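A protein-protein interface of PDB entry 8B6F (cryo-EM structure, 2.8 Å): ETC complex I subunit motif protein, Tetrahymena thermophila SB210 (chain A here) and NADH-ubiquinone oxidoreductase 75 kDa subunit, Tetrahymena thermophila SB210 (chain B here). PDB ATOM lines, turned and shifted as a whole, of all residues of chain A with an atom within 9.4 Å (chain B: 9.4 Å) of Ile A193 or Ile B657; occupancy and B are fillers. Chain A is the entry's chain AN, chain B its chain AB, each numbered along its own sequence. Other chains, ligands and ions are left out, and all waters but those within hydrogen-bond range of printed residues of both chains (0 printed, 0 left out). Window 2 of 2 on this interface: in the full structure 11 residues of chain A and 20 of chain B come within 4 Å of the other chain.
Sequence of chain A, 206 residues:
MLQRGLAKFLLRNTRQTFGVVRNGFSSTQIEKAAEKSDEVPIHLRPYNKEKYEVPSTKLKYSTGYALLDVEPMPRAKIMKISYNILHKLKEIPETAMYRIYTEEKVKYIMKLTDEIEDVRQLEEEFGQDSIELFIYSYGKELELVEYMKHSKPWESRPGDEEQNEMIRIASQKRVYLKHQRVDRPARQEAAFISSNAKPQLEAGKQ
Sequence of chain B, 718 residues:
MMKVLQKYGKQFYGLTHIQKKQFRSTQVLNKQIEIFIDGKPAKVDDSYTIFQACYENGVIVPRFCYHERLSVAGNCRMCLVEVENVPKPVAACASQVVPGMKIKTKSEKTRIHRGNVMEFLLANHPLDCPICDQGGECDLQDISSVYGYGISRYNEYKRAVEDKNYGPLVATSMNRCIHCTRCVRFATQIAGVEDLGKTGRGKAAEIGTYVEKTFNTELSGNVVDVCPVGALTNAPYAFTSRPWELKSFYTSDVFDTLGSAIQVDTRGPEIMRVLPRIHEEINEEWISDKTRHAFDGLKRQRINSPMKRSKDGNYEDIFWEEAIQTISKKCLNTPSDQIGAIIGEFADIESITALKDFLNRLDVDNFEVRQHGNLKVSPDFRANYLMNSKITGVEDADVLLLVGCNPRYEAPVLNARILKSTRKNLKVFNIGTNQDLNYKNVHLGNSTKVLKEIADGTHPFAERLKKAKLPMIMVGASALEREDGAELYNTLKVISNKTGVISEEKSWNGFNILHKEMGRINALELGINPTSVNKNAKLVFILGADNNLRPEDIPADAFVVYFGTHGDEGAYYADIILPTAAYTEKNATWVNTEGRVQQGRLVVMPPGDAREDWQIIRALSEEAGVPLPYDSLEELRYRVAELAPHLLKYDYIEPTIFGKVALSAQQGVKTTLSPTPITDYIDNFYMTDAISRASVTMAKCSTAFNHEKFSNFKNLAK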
ATOM      1  N   GLU A 189     -10.780  20.018  10.070  1.00  0.00           N
ATOM      2  CA  GLU A 189     -10.708  20.537  11.428  1.00  0.00           C
ATOM      3  C   GLU A 189     -10.292  19.424  12.382  1.00  0.00           C
ATOM      4  O   GLU A 189     -11.019  18.440  12.553  1.00  0.00           O
ATOM      5  CB  GLU A 189     -12.058  21.118  11.838  1.00  0.00           C
ATOM      6  CG  GLU A 189     -12.626  22.128  10.856  1.00  0.00           C
ATOM      7  CD  GLU A 189     -11.721  23.326  10.661  1.00  0.00           C
ATOM      8  OE1 GLU A 189     -10.804  23.518  11.484  1.00  0.00           O
ATOM      9  OE2 GLU A 189     -11.926  24.074   9.682  1.00  0.00           O
ATOM     10  N   ALA A 190      -9.127  19.580  13.003  1.00  0.00           N
ATOM     11  CA  ALA A 190      -8.645  18.581  13.947  1.00  0.00           C
ATOM     12  C   ALA A 190      -9.540  18.550  15.178  1.00  0.00           C
ATOM     13  O   ALA A 190      -9.885  19.595  15.736  1.00  0.00           O
ATOM     14  CB  ALA A 190      -7.203  18.882  14.347  1.00  0.00           C
ATOM     15  N   ALA A 191      -9.916  17.348  15.602  1.00  0.00           N
ATOM     16  CA  ALA A 191     -10.764  17.150  16.767  1.00  0.00           C
ATOM     17  C   ALA A 191      -9.944  16.547  17.899  1.00  0.00           C
ATOM     18  O   ALA A 191      -9.089  15.688  17.668  1.00  0.00           O
ATOM     19  CB  ALA A 191     -11.947  16.237  16.437  1.00  0.00           C
ATOM     20  N   PHE A 192     -10.203  17.009  19.120  1.00  0.00           N
ATOM     21  CA  PHE A 192      -9.509  16.534  20.307  1.00  0.00           C
ATOM     22  C   PHE A 192     -10.522  16.017  21.316  1.00  0.00           C
ATOM     23  O   PHE A 192     -11.567  16.637  21.534  1.00  0.00           O
ATOM     24  CB  PHE A 192      -8.664  17.645  20.935  1.00  0.00           C
ATOM     25  CG  PHE A 192      -7.673  18.256  19.989  1.00  0.00           C
ATOM     26  CD1 PHE A 192      -6.457  17.640  19.748  1.00  0.00           C
ATOM     27  CD2 PHE A 192      -7.957  19.448  19.344  1.00  0.00           C
ATOM     28  CE1 PHE A 192      -5.541  18.199  18.879  1.00  0.00           C
ATOM     29  CE2 PHE A 192      -7.046  20.014  18.472  1.00  0.00           C
ATOM     30  CZ  PHE A 192      -5.837  19.388  18.240  1.00  0.00           C
ATOM     31  N   ILE A 193     -10.209  14.876  21.928  1.00  0.00           N
ATOM     32  CA  ILE A 193     -11.101  14.294  22.923  1.00  0.00           C
ATOM     33  C   ILE A 193     -11.144  15.195  24.149  1.00  0.00           C
ATOM     34  O   ILE A 193     -10.104  15.611  24.674  1.00  0.00           O
ATOM     35  CB  ILE A 193     -10.650  12.869  23.283  1.00  0.00           C
ATOM     36  CG1 ILE A 193     -11.652  12.203  24.231  1.00  0.00           C
ATOM     37  CG2 ILE A 193      -9.264  12.877  23.915  1.00  0.00           C
ATOM     38  CD1 ILE A 193     -13.045  12.049  23.657  1.00  0.00           C
ATOM     39  N   SER A 194     -12.354  15.508  24.605  1.00  0.00           N
ATOM     40  CA  SER A 194     -12.516  16.397  25.745  1.00  0.00           C
ATOM     41  C   SER A 194     -11.947  15.759  27.007  1.00  0.00           C
ATOM     42  O   SER A 194     -12.037  14.545  27.204  1.00  0.00           O
ATOM     43  CB  SER A 194     -13.993  16.732  25.951  1.00  0.00           C
ATOM     44  OG  SER A 194     -14.536  17.370  24.808  1.00  0.00           O
ATOM     45  N   SER A 195     -11.361  16.590  27.862  1.00  0.00           N
ATOM     46  CA  SER A 195     -10.783  16.124  29.117  1.00  0.00           C
ATOM     47  C   SER A 195      -9.738  15.041  28.868  1.00  0.00           C
ATOM     48  O   SER A 195      -8.559  15.334  28.667  1.00  0.00           O
ATOM     49  CB  SER A 195     -11.882  15.598  30.046  1.00  0.00           C
ATOM     50  OG  SER A 195     -11.350  15.217  31.304  1.00  0.00           O
ATOM     51  N   PHE B 381       0.714   6.497  20.351  1.00  0.00           N
ATOM     52  CA  PHE B 381      -0.224   7.279  19.560  1.00  0.00           C
ATOM     53  C   PHE B 381       0.384   7.612  18.205  1.00  0.00           C
ATOM     54  O   PHE B 381       1.568   7.941  18.108  1.00  0.00           O
ATOM     55  CB  PHE B 381      -0.604   8.573  20.280  1.00  0.00           C
ATOM     56  CG  PHE B 381      -1.440   8.362  21.505  1.00  0.00           C
ATOM     57  CD1 PHE B 381      -2.801   8.142  21.398  1.00  0.00           C
ATOM     58  CD2 PHE B 381      -0.867   8.398  22.765  1.00  0.00           C
ATOM     59  CE1 PHE B 381      -3.577   7.954  22.525  1.00  0.00           C
ATOM     60  CE2 PHE B 381      -1.638   8.209  23.895  1.00  0.00           C
ATOM     61  CZ  PHE B 381      -2.994   7.987  23.776  1.00  0.00           C
ATOM     62  N   ARG B 382      -0.436   7.520  17.156  1.00  0.00           N
ATOM     63  CA  ARG B 382       0.030   7.911  15.831  1.00  0.00           C
ATOM     64  C   ARG B 382       0.331   9.401  15.769  1.00  0.00           C
ATOM     65  O   ARG B 382       1.196   9.826  14.998  1.00  0.00           O
ATOM     66  CB  ARG B 382      -1.012   7.532  14.779  1.00  0.00           C
ATOM     67  CG  ARG B 382      -1.353   6.054  14.777  1.00  0.00           C
ATOM     68  CD  ARG B 382      -2.452   5.717  13.784  1.00  0.00           C
ATOM     69  NE  ARG B 382      -1.984   5.741  12.402  1.00  0.00           N
ATOM     70  CZ  ARG B 382      -2.146   6.755  11.560  1.00  0.00           C
ATOM     71  NH1 ARG B 382      -2.758   7.871  11.925  1.00  0.00           N
ATOM     72  NH2 ARG B 382      -1.684   6.645  10.318  1.00  0.00           N
ATOM     73  N   ALA B 383      -0.350  10.201  16.588  1.00  0.00           N
ATOM     74  CA  ALA B 383      -0.158  11.645  16.542  1.00  0.00           C
ATOM     75  C   ALA B 383       1.248  12.048  16.964  1.00  0.00           C
ATOM     76  O   ALA B 383       1.745  13.092  16.528  1.00  0.00           O
ATOM     77  CB  ALA B 383      -1.188  12.342  17.429  1.00  0.00           C
ATOM     78  N   ASN B 388       0.843  15.528  12.090  1.00  0.00           N
ATOM     79  CA  ASN B 388      -0.540  15.832  12.438  1.00  0.00           C
ATOM     80  C   ASN B 388      -1.206  16.647  11.339  1.00  0.00           C
ATOM     81  O   ASN B 388      -2.336  16.360  10.929  1.00  0.00           O
ATOM     82  CB  ASN B 388      -0.582  16.587  13.766  1.00  0.00           C
ATOM     83  CG  ASN B 388      -0.023  15.774  14.914  1.00  0.00           C
ATOM     84  OD1 ASN B 388      -0.766  15.125  15.648  1.00  0.00           O
ATOM     85  ND2 ASN B 388       1.295  15.800  15.073  1.00  0.00           N
ATOM     86  N   ILE B 502      -0.475  23.446  18.922  1.00  0.00           N
ATOM     87  CA  ILE B 502      -1.593  22.530  19.113  1.00  0.00           C
ATOM     88  C   ILE B 502      -2.698  23.301  19.820  1.00  0.00           C
ATOM     89  O   ILE B 502      -2.716  23.391  21.052  1.00  0.00           O
ATOM     90  CB  ILE B 502      -1.181  21.286  19.917  1.00  0.00           C
ATOM     91  CG1 ILE B 502       0.094  20.673  19.330  1.00  0.00           C
ATOM     92  CG2 ILE B 502      -2.313  20.267  19.915  1.00  0.00           C
ATOM     93  CD1 ILE B 502       0.642  19.507  20.121  1.00  0.00           C
ATOM     94  N   GLU B 504      -6.804  24.000  20.459  1.00  0.00           N
ATOM     95  CA  GLU B 504      -8.163  23.478  20.373  1.00  0.00           C
ATOM     96  C   GLU B 504      -9.106  24.491  19.736  1.00  0.00           C
ATOM     97  O   GLU B 504      -9.969  24.119  18.932  1.00  0.00           O
ATOM     98  CB  GLU B 504      -8.659  23.087  21.765  1.00  0.00           C
ATOM     99  CG  GLU B 504      -9.721  21.993  21.771  1.00  0.00           C
ATOM    100  CD  GLU B 504     -11.045  22.444  21.190  1.00  0.00           C
ATOM    101  OE1 GLU B 504     -11.352  23.652  21.265  1.00  0.00           O
ATOM    102  OE2 GLU B 504     -11.783  21.587  20.659  1.00  0.00           O
ATOM    103  N   ASN B 509      -3.282  21.282  14.679  1.00  0.00           N
ATOM    104  CA  ASN B 509      -2.178  20.521  15.263  1.00  0.00           C
ATOM    105  C   ASN B 509      -1.019  20.604  14.273  1.00  0.00           C
ATOM    106  O   ASN B 509      -0.885  19.756  13.388  1.00  0.00           O
ATOM    107  CB  ASN B 509      -2.590  19.081  15.542  1.00  0.00           C
ATOM    108  CG  ASN B 509      -1.534  18.309  16.309  1.00  0.00           C
ATOM    109  OD1 ASN B 509      -0.349  18.637  16.259  1.00  0.00           O
ATOM    110  ND2 ASN B 509      -1.959  17.273  17.020  1.00  0.00           N
ATOM    111  N   GLU B 654      -6.519   8.175   8.490  1.00  0.00           N
ATOM    112  CA  GLU B 654      -7.497   8.024   9.559  1.00  0.00           C
ATOM    113  C   GLU B 654      -7.273   9.101  10.614  1.00  0.00           C
ATOM    114  O   GLU B 654      -6.172   9.186  11.168  1.00  0.00           O
ATOM    115  CB  GLU B 654      -7.385   6.643  10.189  1.00  0.00           C
ATOM    116  CG  GLU B 654      -8.502   6.315  11.167  1.00  0.00           C
ATOM    117  CD  GLU B 654      -9.845   6.152  10.483  1.00  0.00           C
ATOM    118  OE1 GLU B 654      -9.863   5.809   9.284  1.00  0.00           O
ATOM    119  OE2 GLU B 654     -10.881   6.368  11.144  1.00  0.00           O
ATOM    120  N   PRO B 655      -8.267   9.931  10.923  1.00  0.00           N
ATOM    121  CA  PRO B 655      -8.058  10.974  11.932  1.00  0.00           C
ATOM    122  C   PRO B 655      -7.901  10.387  13.324  1.00  0.00           C
ATOM    123  O   PRO B 655      -8.405   9.305  13.633  1.00  0.00           O
ATOM    124  CB  PRO B 655      -9.326  11.829  11.827  1.00  0.00           C
ATOM    125  CG  PRO B 655     -10.356  10.900  11.311  1.00  0.00           C
ATOM    126  CD  PRO B 655      -9.643   9.949  10.395  1.00  0.00           C
ATOM    127  N   THR B 656      -7.182  11.121  14.170  1.00  0.00           N
ATOM    128  CA  THR B 656      -6.971  10.746  15.561  1.00  0.00           C
ATOM    129  C   THR B 656      -7.403  11.895  16.460  1.00  0.00           C
ATOM    130  O   THR B 656      -7.112  13.059  16.172  1.00  0.00           O
ATOM    131  CB  THR B 656      -5.500  10.388  15.826  1.00  0.00           C
ATOM    132  OG1 THR B 656      -5.335   9.991  17.194  1.00  0.00           O
ATOM    133  CG2 THR B 656      -4.587  11.572  15.528  1.00  0.00           C
ATOM    134  N   ILE B 657      -8.101  11.563  17.546  1.00  0.00           N
ATOM    135  CA  ILE B 657      -8.607  12.563  18.480  1.00  0.00           C
ATOM    136  C   ILE B 657      -7.765  12.638  19.749  1.00  0.00           C
ATOM    137  O   ILE B 657      -8.135  13.347  20.689  1.00  0.00           O
ATOM    138  CB  ILE B 657     -10.082  12.305  18.827  1.00  0.00           C
ATOM    139  CG1 ILE B 657     -10.257  10.907  19.426  1.00  0.00           C
ATOM    140  CG2 ILE B 657     -10.948  12.470  17.589  1.00  0.00           C
ATOM    141  CD1 ILE B 657     -11.619  10.672  20.036  1.00  0.00           C
ATOM    142  N   PHE B 658      -6.642  11.923  19.802  1.00  0.00           N
ATOM    143  CA  PHE B 658      -5.764  11.921  20.965  1.00  0.00           C
ATOM    144  C   PHE B 658      -4.483  12.708  20.722  1.00  0.00           C
ATOM    145  O   PHE B 658      -3.477  12.474  21.399  1.00  0.00           O
ATOM    146  CB  PHE B 658      -5.430  10.484  21.370  1.00  0.00           C
ATOM    147  CG  PHE B 658      -6.563   9.763  22.038  1.00  0.00           C
ATOM    148  CD1 PHE B 658      -7.593   9.221  21.291  1.00  0.00           C
ATOM    149  CD2 PHE B 658      -6.589   9.615  23.413  1.00  0.00           C
ATOM    150  CE1 PHE B 658      -8.635   8.553  21.902  1.00  0.00           C
ATOM    151  CE2 PHE B 658      -7.628   8.948  24.031  1.00  0.00           C
ATOM    152  CZ  PHE B 658      -8.652   8.417  23.274  1.00  0.00           C
ATOM    153  N   GLY B 659      -4.496  13.638  19.766  1.00  0.00           N
ATOM    154  CA  GLY B 659      -3.286  14.389  19.473  1.00  0.00           C
ATOM    155  C   GLY B 659      -2.823  15.224  20.649  1.00  0.00           C
ATOM    156  O   GLY B 659      -1.642  15.223  21.003  1.00  0.00           O
ATOM    157  N   LYS B 660      -3.750  15.952  21.274  1.00  0.00           N
ATOM    158  CA  LYS B 660      -3.379  16.801  22.401  1.00  0.00           C
ATOM    159  C   LYS B 660      -2.873  15.968  23.571  1.00  0.00           C
ATOM    160  O   LYS B 660      -1.879  16.324  24.215  1.00  0.00           O
ATOM    161  CB  LYS B 660      -4.569  17.657  22.827  1.00  0.00           C
ATOM    162  CG  LYS B 660      -4.216  18.734  23.842  1.00  0.00           C
ATOM    163  CD  LYS B 660      -5.459  19.355  24.459  1.00  0.00           C
ATOM    164  CE  LYS B 660      -6.321  20.048  23.415  1.00  0.00           C
ATOM    165  NZ  LYS B 660      -7.515  20.683  24.039  1.00  0.00           N
ATOM    166  N   VAL B 661      -3.548  14.854  23.865  1.00  0.00           N
ATOM    167  CA  VAL B 661      -3.112  13.986  24.955  1.00  0.00           C
ATOM    168  C   VAL B 661      -1.730  13.421  24.664  1.00  0.00           C
ATOM    169  O   VAL B 661      -0.855  13.397  25.537  1.00  0.00           O
ATOM    170  CB  VAL B 661      -4.144  12.865  25.188  1.00  0.00           C
ATOM    171  CG1 VAL B 661      -3.683  11.927  26.298  1.00  0.00           C
ATOM    172  CG2 VAL B 661      -5.508  13.452  25.518  1.00  0.00           C
ATOM    173  N   ALA B 662      -1.509  12.958  23.432  1.00  0.00           N
ATOM    174  CA  ALA B 662      -0.232  12.344  23.091  1.00  0.00           C
ATOM    175  C   ALA B 662       0.911  13.348  23.171  1.00  0.00           C
ATOM    176  O   ALA B 662       1.990  13.031  23.682  1.00  0.00           O
ATOM    177  CB  ALA B 662      -0.305  11.733  21.692  1.00  0.00           C
ATOM    178  N   LEU B 663       0.694  14.561  22.672  1.00  0.00           N
ATOM    179  CA  LEU B 663       1.746  15.564  22.597  1.00  0.00           C
ATOM    180  C   LEU B 663       1.789  16.479  23.812  1.00  0.00           C
ATOM    181  O   LEU B 663       2.609  17.402  23.845  1.00  0.00           O
ATOM    182  CB  LEU B 663       1.575  16.405  21.327  1.00  0.00           C
ATOM    183  CG  LEU B 663       1.707  15.633  20.010  1.00  0.00           C
ATOM    184  CD1 LEU B 663       1.350  16.508  18.823  1.00  0.00           C
ATOM    185  CD2 LEU B 663       3.113  15.080  19.850  1.00  0.00           C
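O of Ile B657 is in hydrogen-bond range of N of Ile A193, at 2.9 Å.
The side-chain hydroxyl of Thr B656 lies close to the backbone NH of Phe B658, at 3.5 Å.
Among the printed residues, pairs that only touch across the chains: Ala A191 with Thr B656 (3.6 Å), Ala A191 with Ile B657 (3.3 Å), Phe A192 with Ile B502 (3.97 Å), Phe A192 with Glu B504 (3.9 Å), Phe A192 with Ile B657 (3.5 Å) and Phe A192 with Lys B660 (3.5 Å).
Of the printed residues of chain B, Ala A191 touches Thr B656 (3.6 Å) and Ile B657 (3.3 Å).
Of the printed residues of chain B, Phe A192 touches Ile B502, Glu B504, Ile B657 and Lys B660.
Of chain B, only Ile B657 comes within 4 Å of Ile A193.
Printed residues of chain A within 4 Å of Ile B502: Phe A192.
Printed residues of chain A within 4 Å of Glu B504: Phe A192 (3.9 Å).
Of the printed residues of chain A, Ile B657 touches Ala A191 (3.3 Å), Phe A192 (3.5 Å) and Ile A193 (2.9 Å).
The nearest residue of chain A that does not touch Ile B657 is Ser A194 (6.1 Å).
The nearest printed residue of chain B that does not touch Phe A192 is Asn B509 (4.1 Å).
Hydrophobic or aromatic side chains of chain B that line the printed part of chain A: Ile B502 and Ile B657.
Of the 7 printed residues of chain A, 3 touch a printed residue of chain B.
Hydrophobic or aromatic side chains of chain A within 4 Å of the printed part of chain B: Phe A192 and Ile A193.
Among the printed residues, 7 pairs touch across the chains.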
